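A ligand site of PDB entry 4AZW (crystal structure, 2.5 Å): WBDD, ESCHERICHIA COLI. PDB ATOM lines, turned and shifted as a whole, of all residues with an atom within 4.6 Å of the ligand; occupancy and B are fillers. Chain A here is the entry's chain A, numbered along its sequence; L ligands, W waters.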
ATOM      1  N   TYR A  29       0.188  -2.311  22.903  1.00  0.00           N
ATOM      2  CA  TYR A  29       0.958  -3.513  22.513  1.00  0.00           C
ATOM      3  C   TYR A  29       1.167  -4.430  23.720  1.00  0.00           C
ATOM      4  O   TYR A  29       0.773  -5.599  23.685  1.00  0.00           O
ATOM      5  CB  TYR A  29       2.290  -3.134  21.829  1.00  0.00           C
ATOM      6  CG  TYR A  29       2.993  -4.319  21.185  1.00  0.00           C
ATOM      7  CD1 TYR A  29       2.685  -4.741  19.885  1.00  0.00           C
ATOM      8  CD2 TYR A  29       3.964  -5.039  21.890  1.00  0.00           C
ATOM      9  CE1 TYR A  29       3.319  -5.830  19.309  1.00  0.00           C
ATOM     10  CE2 TYR A  29       4.619  -6.122  21.324  1.00  0.00           C
ATOM     11  CZ  TYR A  29       4.293  -6.516  20.036  1.00  0.00           C
ATOM     12  OH  TYR A  29       4.949  -7.592  19.505  1.00  0.00           O
ATOM     13  N   GLN A  30       1.762  -3.880  24.781  1.00  0.00           N
ATOM     14  CA  GLN A  30       2.077  -4.624  26.005  1.00  0.00           C
ATOM     15  C   GLN A  30       1.016  -4.450  27.102  1.00  0.00           C
ATOM     16  O   GLN A  30       0.199  -3.553  27.059  1.00  0.00           O
ATOM     17  CB  GLN A  30       3.396  -4.126  26.585  1.00  0.00           C
ATOM     18  CG  GLN A  30       4.601  -4.245  25.681  1.00  0.00           C
ATOM     19  CD  GLN A  30       5.777  -3.433  26.189  1.00  0.00           C
ATOM     20  OE1 GLN A  30       5.598  -2.434  26.890  1.00  0.00           O
ATOM     21  NE2 GLN A  30       6.984  -3.839  25.825  1.00  0.00           N
ATOM     22  N   ARG A  44      -0.240  -8.419  23.505  1.00  0.00           N
ATOM     23  CA  ARG A  44       0.739  -9.417  23.966  1.00  0.00           C
ATOM     24  C   ARG A  44       0.754  -9.596  25.504  1.00  0.00           C
ATOM     25  O   ARG A  44       0.913  -8.614  26.253  1.00  0.00           O
ATOM     26  CB  ARG A  44       2.138  -9.011  23.489  1.00  0.00           C
ATOM     27  CG  ARG A  44       2.362  -9.211  21.997  1.00  0.00           C
ATOM     28  CD  ARG A  44       3.198 -10.442  21.671  1.00  0.00           C
ATOM     29  NE  ARG A  44       4.464 -10.028  21.077  1.00  0.00           N
ATOM     30  CZ  ARG A  44       5.563 -10.772  21.015  1.00  0.00           C
ATOM     31  NH1 ARG A  44       5.636 -12.020  21.489  1.00  0.00           N
ATOM     32  NH2 ARG A  44       6.638 -10.224  20.448  1.00  0.00           N
ATOM     33  N   ARG A  49       7.862 -14.232  28.388  1.00  0.00           N
ATOM     34  CA  ARG A  49       9.095 -13.638  27.923  1.00  0.00           C
ATOM     35  C   ARG A  49       9.815 -12.874  29.025  1.00  0.00           C
ATOM     36  O   ARG A  49      11.027 -12.731  28.971  1.00  0.00           O
ATOM     37  CB  ARG A  49       8.862 -12.674  26.767  1.00  0.00           C
ATOM     38  CG  ARG A  49       8.165 -13.248  25.522  1.00  0.00           C
ATOM     39  CD  ARG A  49       7.090 -12.274  25.004  1.00  0.00           C
ATOM     40  NE  ARG A  49       7.649 -11.192  24.212  1.00  0.00           N
ATOM     41  CZ  ARG A  49       7.170  -9.941  24.101  1.00  0.00           C
ATOM     42  NH1 ARG A  49       6.066  -9.528  24.742  1.00  0.00           N
ATOM     43  NH2 ARG A  49       7.831  -9.085  23.337  1.00  0.00           N
ATOM     44  N   LEU A  73      15.270  -1.435  23.515  1.00  0.00           N
ATOM     45  CA  LEU A  73      15.157  -0.907  22.173  1.00  0.00           C
ATOM     46  C   LEU A  73      13.751  -1.198  21.603  1.00  0.00           C
ATOM     47  O   LEU A  73      13.403  -2.351  21.315  1.00  0.00           O
ATOM     48  CB  LEU A  73      16.239  -1.556  21.295  1.00  0.00           C
ATOM     49  CG  LEU A  73      17.668  -1.043  21.486  1.00  0.00           C
ATOM     50  CD1 LEU A  73      18.685  -1.812  20.659  1.00  0.00           C
ATOM     51  CD2 LEU A  73      17.688   0.432  21.132  1.00  0.00           C
ATOM     52  N   GLY A  74      12.965  -0.153  21.376  1.00  0.00           N
ATOM     53  CA  GLY A  74      11.577  -0.312  20.985  1.00  0.00           C
ATOM     54  C   GLY A  74      10.745  -0.747  22.180  1.00  0.00           C
ATOM     55  O   GLY A  74      10.057  -1.778  22.144  1.00  0.00           O
ATOM     56  N   ALA A  76       8.068   0.339  23.620  1.00  0.00           N
ATOM     57  CA  ALA A  76       6.604   0.334  23.621  1.00  0.00           C
ATOM     58  C   ALA A  76       6.088   1.053  24.876  1.00  0.00           C
ATOM     59  O   ALA A  76       6.463   2.187  25.159  1.00  0.00           O
ATOM     60  CB  ALA A  76       6.063  -1.099  23.582  1.00  0.00           C
ATOM     61  N   PHE A  80       8.800  -4.092  29.950  1.00  0.00           N
ATOM     62  CA  PHE A  80      10.047  -4.791  30.269  1.00  0.00           C
ATOM     63  C   PHE A  80      11.031  -3.864  30.993  1.00  0.00           C
ATOM     64  O   PHE A  80      11.720  -4.316  31.854  1.00  0.00           O
ATOM     65  CB  PHE A  80      10.691  -5.460  29.028  1.00  0.00           C
ATOM     66  CG  PHE A  80       9.842  -6.506  28.395  1.00  0.00           C
ATOM     67  CD1 PHE A  80       9.816  -7.795  28.896  1.00  0.00           C
ATOM     68  CD2 PHE A  80       9.036  -6.207  27.310  1.00  0.00           C
ATOM     69  CE1 PHE A  80       9.013  -8.781  28.317  1.00  0.00           C
ATOM     70  CE2 PHE A  80       8.239  -7.174  26.728  1.00  0.00           C
ATOM     71  CZ  PHE A  80       8.215  -8.460  27.251  1.00  0.00           C
ATOM     72  N   ILE A  94      13.930   3.243  24.524  1.00  0.00           N
ATOM     73  CA  ILE A  94      13.885   3.975  23.259  1.00  0.00           C
ATOM     74  C   ILE A  94      12.689   3.470  22.484  1.00  0.00           C
ATOM     75  O   ILE A  94      12.482   2.261  22.413  1.00  0.00           O
ATOM     76  CB  ILE A  94      15.128   3.675  22.412  1.00  0.00           C
ATOM     77  CG1 ILE A  94      16.384   4.192  23.115  1.00  0.00           C
ATOM     78  CG2 ILE A  94      14.975   4.269  21.025  1.00  0.00           C
ATOM     79  CD1 ILE A  94      16.349   5.671  23.423  1.00  0.00           C
ATOM     80  N   ASP A  95      11.886   4.384  21.959  1.00  0.00           N
ATOM     81  CA  ASP A  95      10.801   4.066  21.044  1.00  0.00           C
ATOM     82  C   ASP A  95      10.685   5.285  20.147  1.00  0.00           C
ATOM     83  O   ASP A  95      10.979   6.381  20.622  1.00  0.00           O
ATOM     84  CB  ASP A  95       9.504   3.753  21.800  1.00  0.00           C
ATOM     85  CG  ASP A  95       8.510   2.928  20.977  1.00  0.00           C
ATOM     86  OD1 ASP A  95       7.891   3.475  20.048  1.00  0.00           O
ATOM     87  OD2 ASP A  95       8.349   1.727  21.268  1.00  0.00           O
ATOM     88  N   PHE A  96      10.332   5.109  18.854  1.00  0.00           N
ATOM     89  CA  PHE A  96      10.175   6.255  17.959  1.00  0.00           C
ATOM     90  C   PHE A  96       8.773   6.886  17.951  1.00  0.00           C
ATOM     91  O   PHE A  96       8.502   7.792  17.185  1.00  0.00           O
ATOM     92  CB  PHE A  96      10.749   6.030  16.542  1.00  0.00           C
ATOM     93  CG  PHE A  96       9.992   5.054  15.674  1.00  0.00           C
ATOM     94  CD1 PHE A  96       8.823   4.428  16.063  1.00  0.00           C
ATOM     95  CD2 PHE A  96      10.488   4.781  14.401  1.00  0.00           C
ATOM     96  CE1 PHE A  96       8.179   3.539  15.220  1.00  0.00           C
ATOM     97  CE2 PHE A  96       9.855   3.899  13.551  1.00  0.00           C
ATOM     98  CZ  PHE A  96       8.702   3.273  13.965  1.00  0.00           C
ATOM     99  N   GLN A  97       7.880   6.410  18.818  1.00  0.00           N
ATOM    100  CA  GLN A  97       6.533   6.967  18.905  1.00  0.00           C
ATOM    101  C   GLN A  97       6.361   7.758  20.180  1.00  0.00           C
ATOM    102  O   GLN A  97       6.461   7.216  21.294  1.00  0.00           O
ATOM    103  CB  GLN A  97       5.483   5.880  18.847  1.00  0.00           C
ATOM    104  CG  GLN A  97       5.522   5.103  17.550  1.00  0.00           C
ATOM    105  CD  GLN A  97       4.183   4.507  17.219  1.00  0.00           C
ATOM    106  OE1 GLN A  97       3.247   5.241  16.894  1.00  0.00           O
ATOM    107  NE2 GLN A  97       4.082   3.176  17.294  1.00  0.00           N
ATOM    108  N   ASN A 100       4.018   6.535  22.924  1.00  0.00           N
ATOM    109  CA  ASN A 100       4.560   5.398  23.671  1.00  0.00           C
ATOM    110  C   ASN A 100       5.392   5.879  24.853  1.00  0.00           C
ATOM    111  O   ASN A 100       5.189   5.428  25.982  1.00  0.00           O
ATOM    112  CB  ASN A 100       5.386   4.489  22.751  1.00  0.00           C
ATOM    113  CG  ASN A 100       4.535   3.504  21.918  1.00  0.00           C
ATOM    114  OD1 ASN A 100       3.317   3.353  22.106  1.00  0.00           O
ATOM    115  ND2 ASN A 100       5.195   2.821  20.987  1.00  0.00           N
ATOM    116  N   GLY A 121      13.290   8.195  19.938  1.00  0.00           N
ATOM    117  CA  GLY A 121      14.482   8.079  19.090  1.00  0.00           C
ATOM    118  C   GLY A 121      14.295   6.914  18.156  1.00  0.00           C
ATOM    119  O   GLY A 121      13.357   6.170  18.315  1.00  0.00           O
ATOM    120  N   ARG A 122      15.190   6.779  17.188  1.00  0.00           N
ATOM    121  CA  ARG A 122      15.244   5.636  16.303  1.00  0.00           C
ATOM    122  C   ARG A 122      16.411   4.764  16.706  1.00  0.00           C
ATOM    123  O   ARG A 122      17.514   5.261  17.043  1.00  0.00           O
ATOM    124  CB  ARG A 122      15.383   6.083  14.860  1.00  0.00           C
ATOM    125  CG  ARG A 122      14.143   6.840  14.337  1.00  0.00           C
ATOM    126  CD  ARG A 122      14.230   7.145  12.843  1.00  0.00           C
ATOM    127  NE  ARG A 122      14.304   5.900  12.074  1.00  0.00           N
ATOM    128  CZ  ARG A 122      13.269   5.245  11.550  1.00  0.00           C
ATOM    129  NH1 ARG A 122      12.017   5.706  11.671  1.00  0.00           N
ATOM    130  NH2 ARG A 122      13.475   4.097  10.889  1.00  0.00           N
ATOM    131  N   ILE A 123      16.155   3.460  16.677  1.00  0.00           N
ATOM    132  CA  ILE A 123      17.137   2.434  17.041  1.00  0.00           C
ATOM    133  C   ILE A 123      18.451   2.554  16.237  1.00  0.00           C
ATOM    134  O   ILE A 123      19.555   2.352  16.803  1.00  0.00           O
ATOM    135  CB  ILE A 123      16.532   1.002  16.842  1.00  0.00           C
ATOM    136  CG1 ILE A 123      15.547   0.669  17.945  1.00  0.00           C
ATOM    137  CG2 ILE A 123      17.626  -0.030  16.815  1.00  0.00           C
ATOM    138  CD1 ILE A 123      14.453  -0.306  17.550  1.00  0.00           C
ATOM    139  N   GLU A 124      18.327   2.895  14.958  1.00  0.00           N
ATOM    140  CA  GLU A 124      19.478   2.994  14.067  1.00  0.00           C
ATOM    141  C   GLU A 124      20.458   4.055  14.582  1.00  0.00           C
ATOM    142  O   GLU A 124      21.675   3.834  14.628  1.00  0.00           O
ATOM    143  CB  GLU A 124      19.072   3.414  12.648  1.00  0.00           C
ATOM    144  CG  GLU A 124      18.038   2.566  11.933  1.00  0.00           C
ATOM    145  CD  GLU A 124      16.587   2.876  12.308  1.00  0.00           C
ATOM    146  OE1 GLU A 124      16.291   3.138  13.490  1.00  0.00           O
ATOM    147  OE2 GLU A 124      15.724   2.815  11.421  1.00  0.00           O
ATOM    148  N   LEU A 141      13.243  -6.815  21.374  1.00  0.00           N
ATOM    149  CA  LEU A 141      12.183  -7.788  21.170  1.00  0.00           C
ATOM    150  C   LEU A 141      11.224  -7.342  20.065  1.00  0.00           C
ATOM    151  O   LEU A 141      10.641  -6.261  20.136  1.00  0.00           O
ATOM    152  CB  LEU A 141      11.426  -8.057  22.473  1.00  0.00           C
ATOM    153  CG  LEU A 141      12.305  -8.234  23.714  1.00  0.00           C
ATOM    154  CD1 LEU A 141      11.470  -8.436  24.972  1.00  0.00           C
ATOM    155  CD2 LEU A 141      13.355  -9.354  23.537  1.00  0.00           C
ATOM    156  N   SER A 142      11.137  -8.134  19.013  1.00  0.00           N
ATOM    157  CA  SER A 142      10.175  -7.903  17.942  1.00  0.00           C
ATOM    158  C   SER A 142      10.272  -6.469  17.422  1.00  0.00           C
ATOM    159  O   SER A 142       9.304  -5.742  17.425  1.00  0.00           O
ATOM    160  CB  SER A 142       8.765  -8.258  18.450  1.00  0.00           C
ATOM    161  OG  SER A 142       8.668  -9.672  18.782  1.00  0.00           O
ATOM    162  N   VAL A 143      11.460  -6.078  16.995  1.00  0.00           N
ATOM    163  CA  VAL A 143      11.693  -4.763  16.447  1.00  0.00           C
ATOM    164  C   VAL A 143      12.648  -4.752  15.265  1.00  0.00           C
ATOM    165  O   VAL A 143      12.510  -3.928  14.366  1.00  0.00           O
ATOM    166  CB  VAL A 143      12.233  -3.813  17.522  1.00  0.00           C
ATOM    167  CG1 VAL A 143      13.719  -4.034  17.777  1.00  0.00           C
ATOM    168  CG2 VAL A 143      11.953  -2.361  17.086  1.00  0.00           C
ATOM    169  N   HIS A 146      11.263  -4.899  11.324  1.00  0.00           N
ATOM    170  CA  HIS A 146      10.867  -3.612  10.711  1.00  0.00           C
ATOM    171  C   HIS A 146      12.080  -2.955  10.095  1.00  0.00           C
ATOM    172  O   HIS A 146      11.984  -2.400   9.001  1.00  0.00           O
ATOM    173  CB  HIS A 146      10.186  -2.686  11.730  1.00  0.00           C
ATOM    174  CG  HIS A 146       8.884  -3.241  12.298  1.00  0.00           C
ATOM    175  ND1 HIS A 146       7.812  -3.595  11.505  1.00  0.00           N
ATOM    176  CD2 HIS A 146       8.492  -3.517  13.630  1.00  0.00           C
ATOM    177  CE1 HIS A 146       6.809  -4.072  12.298  1.00  0.00           C
ATOM    178  NE2 HIS A 146       7.226  -4.030  13.597  1.00  0.00           N
ATOM    179  N   ILE A 147      13.222  -3.044  10.768  1.00  0.00           N
ATOM    180  CA  ILE A 147      14.429  -2.418  10.320  1.00  0.00           C
ATOM    181  C   ILE A 147      15.034  -3.195   9.126  1.00  0.00           C
ATOM    182  O   ILE A 147      15.600  -2.568   8.220  1.00  0.00           O
ATOM    183  CB  ILE A 147      15.431  -2.258  11.463  1.00  0.00           C
ATOM    184  CG1 ILE A 147      14.810  -1.488  12.655  1.00  0.00           C
ATOM    185  CG2 ILE A 147      16.676  -1.525  11.027  1.00  0.00           C
ATOM    186  CD1 ILE A 147      15.793  -1.349  13.821  1.00  0.00           C
ATOM    187  N   GLU A 173      14.365 -11.115  20.530  1.00  0.00           N
ATOM    188  CA  GLU A 173      13.274 -11.960  20.039  1.00  0.00           C
ATOM    189  C   GLU A 173      12.991 -11.534  18.614  1.00  0.00           C
ATOM    190  O   GLU A 173      12.620 -10.407  18.398  1.00  0.00           O
ATOM    191  CB  GLU A 173      12.012 -11.726  20.838  1.00  0.00           C
ATOM    192  CG  GLU A 173      10.841 -12.557  20.351  1.00  0.00           C
ATOM    193  CD  GLU A 173       9.514 -12.103  20.909  1.00  0.00           C
ATOM    194  OE1 GLU A 173       9.280 -10.881  21.045  1.00  0.00           O
ATOM    195  OE2 GLU A 173       8.656 -12.994  21.147  1.00  0.00           O
HETATM  196  N1  LIG L   1       9.789  -4.509  22.511  1.00  0.00           N
HETATM  197  C1  LIG L   1       8.340  -4.521  22.739  1.00  0.00           C
HETATM  198  C2  LIG L   1       7.846  -5.909  22.979  1.00  0.00           C
HETATM  199  O1  LIG L   1       8.284  -6.837  22.268  1.00  0.00           O
HETATM  200  O2  LIG L   1       6.969  -6.090  23.862  1.00  0.00           O
HETATM  201  C3  LIG L   1       7.476  -3.940  21.600  1.00  0.00           C
HETATM  202  C4  LIG L   1       7.634  -4.528  20.193  1.00  0.00           C
HETATM  203  S1  LIG L   1       6.781  -3.633  19.049  1.00  0.00           S
HETATM  204  C5  LIG L   1       6.148  -4.746  17.971  1.00  0.00           C
HETATM  205  C6  LIG L   1       7.727  -2.589  18.143  1.00  0.00           C
HETATM  206  C7  LIG L   1       8.030  -1.276  18.851  1.00  0.00           C
HETATM  207  O3  LIG L   1       9.194  -0.725  18.264  1.00  0.00           O
HETATM  208  C8  LIG L   1       6.948  -0.218  18.681  1.00  0.00           C
HETATM  209  O4  LIG L   1       6.652   0.293  19.960  1.00  0.00           O
HETATM  210  C9  LIG L   1       7.539   0.820  17.750  1.00  0.00           C
HETATM  211  O5  LIG L   1       7.196   2.153  18.098  1.00  0.00           O
HETATM  212  C10 LIG L   1       9.023   0.628  17.923  1.00  0.00           C
HETATM  213  N2  LIG L   1       9.870   0.763  16.728  1.00  0.00           N
HETATM  214  C11 LIG L   1       9.769   0.161  15.532  1.00  0.00           C
HETATM  215  N3  LIG L   1      10.791   0.543  14.713  1.00  0.00           N
HETATM  216  C12 LIG L   1      11.547   1.393  15.403  1.00  0.00           C
HETATM  217  C13 LIG L   1      12.771   2.157  15.170  1.00  0.00           C
HETATM  218  N4  LIG L   1      13.392   2.105  13.974  1.00  0.00           N
HETATM  219  N5  LIG L   1      13.232   2.934  16.152  1.00  0.00           N
HETATM  220  C14 LIG L   1      12.641   3.008  17.342  1.00  0.00           C
HETATM  221  N6  LIG L   1      11.538   2.347  17.641  1.00  0.00           N
HETATM  222  C15 LIG L   1      10.952   1.543  16.715  1.00  0.00           C
HETATM  223  O   HOH W   1      13.034  -4.228  22.831  1.00  0.00           O
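An oxygen (O1) of the ligand lies within salt-bridge range of the guanidinium group (NH2) of Arg 49 (2.5 Å).
N1 of the ligand lies within hydrogen-bond range of O of Gly 74 (2.8 Å).
N of Phe 96 lies within hydrogen-bond range of N6 of the ligand, at 3.2 Å.
The side-chain carboxylate (OD1) of Asp 95 lies within hydrogen-bond range of an oxygen (O5) of the ligand, at 2.5 Å.
The side-chain amide nitrogen (NE2) of Gln 30 is in hydrogen-bond range of an oxygen (O2) of the ligand (3.0 Å).
The backbone NH (N) of Ile 123 sits at hydrogen-bond distance from a nitrogen (N5) of the ligand, 3.0 Å away.
The side-chain amide nitrogen (ND2) of Asn 100 sits at hydrogen-bond distance from an oxygen (O4) of the ligand, at 3.1 Å.
O of Leu 141 lies within hydrogen-bond range of N1 of the ligand (3.1 Å).
The side-chain amide nitrogen of Gln 97 is in hydrogen-bond range of an oxygen (O5) of the ligand, at 3.4 Å.
The side-chain carboxylate (OE1) of Glu 124 is in hydrogen-bond range of a nitrogen (N4) of the ligand.
The guanidinium group (NE) of Arg 44 sits at hydrogen-bond distance from the side-chain hydroxyl (OH) of Tyr 29 (2.9 Å).
The backbone carbonyl oxygen (O) of Gly 121 lies close to the backbone NH (N) of Phe 96.
OD2 of Asp 95 is in hydrogen-bond range of N of Ala 76, 2.7 Å away.
The side-chain carboxylate of Glu 124 is in salt-bridge range of the guanidinium group of Arg 122, at 2.6 Å.
The side-chain carboxylate (OE1) of Glu 173 sits at hydrogen-bond distance from the side-chain hydroxyl (OG) of Ser 142, at 2.6 Å.
OG of Ser 142 sits at hydrogen-bond distance from NH2 of Arg 44 (2.7 Å).
The backbone NH (N) of Gly 121 is in hydrogen-bond range of the backbone carbonyl oxygen (O) of Asp 95, at 3.0 Å.
OD1 of Asp 95 lies within hydrogen-bond range of N of Gln 97.
A sulfur (S1) of the ligand sits close to the backbone carbonyl oxygen of Ser 142.
Merely in contact with the ligand: Tyr 29, Phe 80, Arg 122, Gly 121, Val 143 and Ala 76.
Hydrophobic or aromatic side chains that line the ligand: Tyr 29, Ala 76, Phe 80, Phe 96, Ile 123, Leu 141 and Val 143.
Within 4 Å of the ligand: Tyr 29, Gln 30, Arg 49, Gly 74, Ala 76, Phe 80, Asp 95, Phe 96, Gln 97, Asn 100, Gly 121, Arg 122, Ile 123, Glu 124, Leu 141, Ser 142 and Val 143.
Water W1 lies within hydrogen-bond range of the backbone carbonyl oxygen (O) of Leu 73 (2.4 Å), the backbone NH (N) of Leu 141 (3.0 Å) and a nitrogen (N1) of the ligand (3.3 Å).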
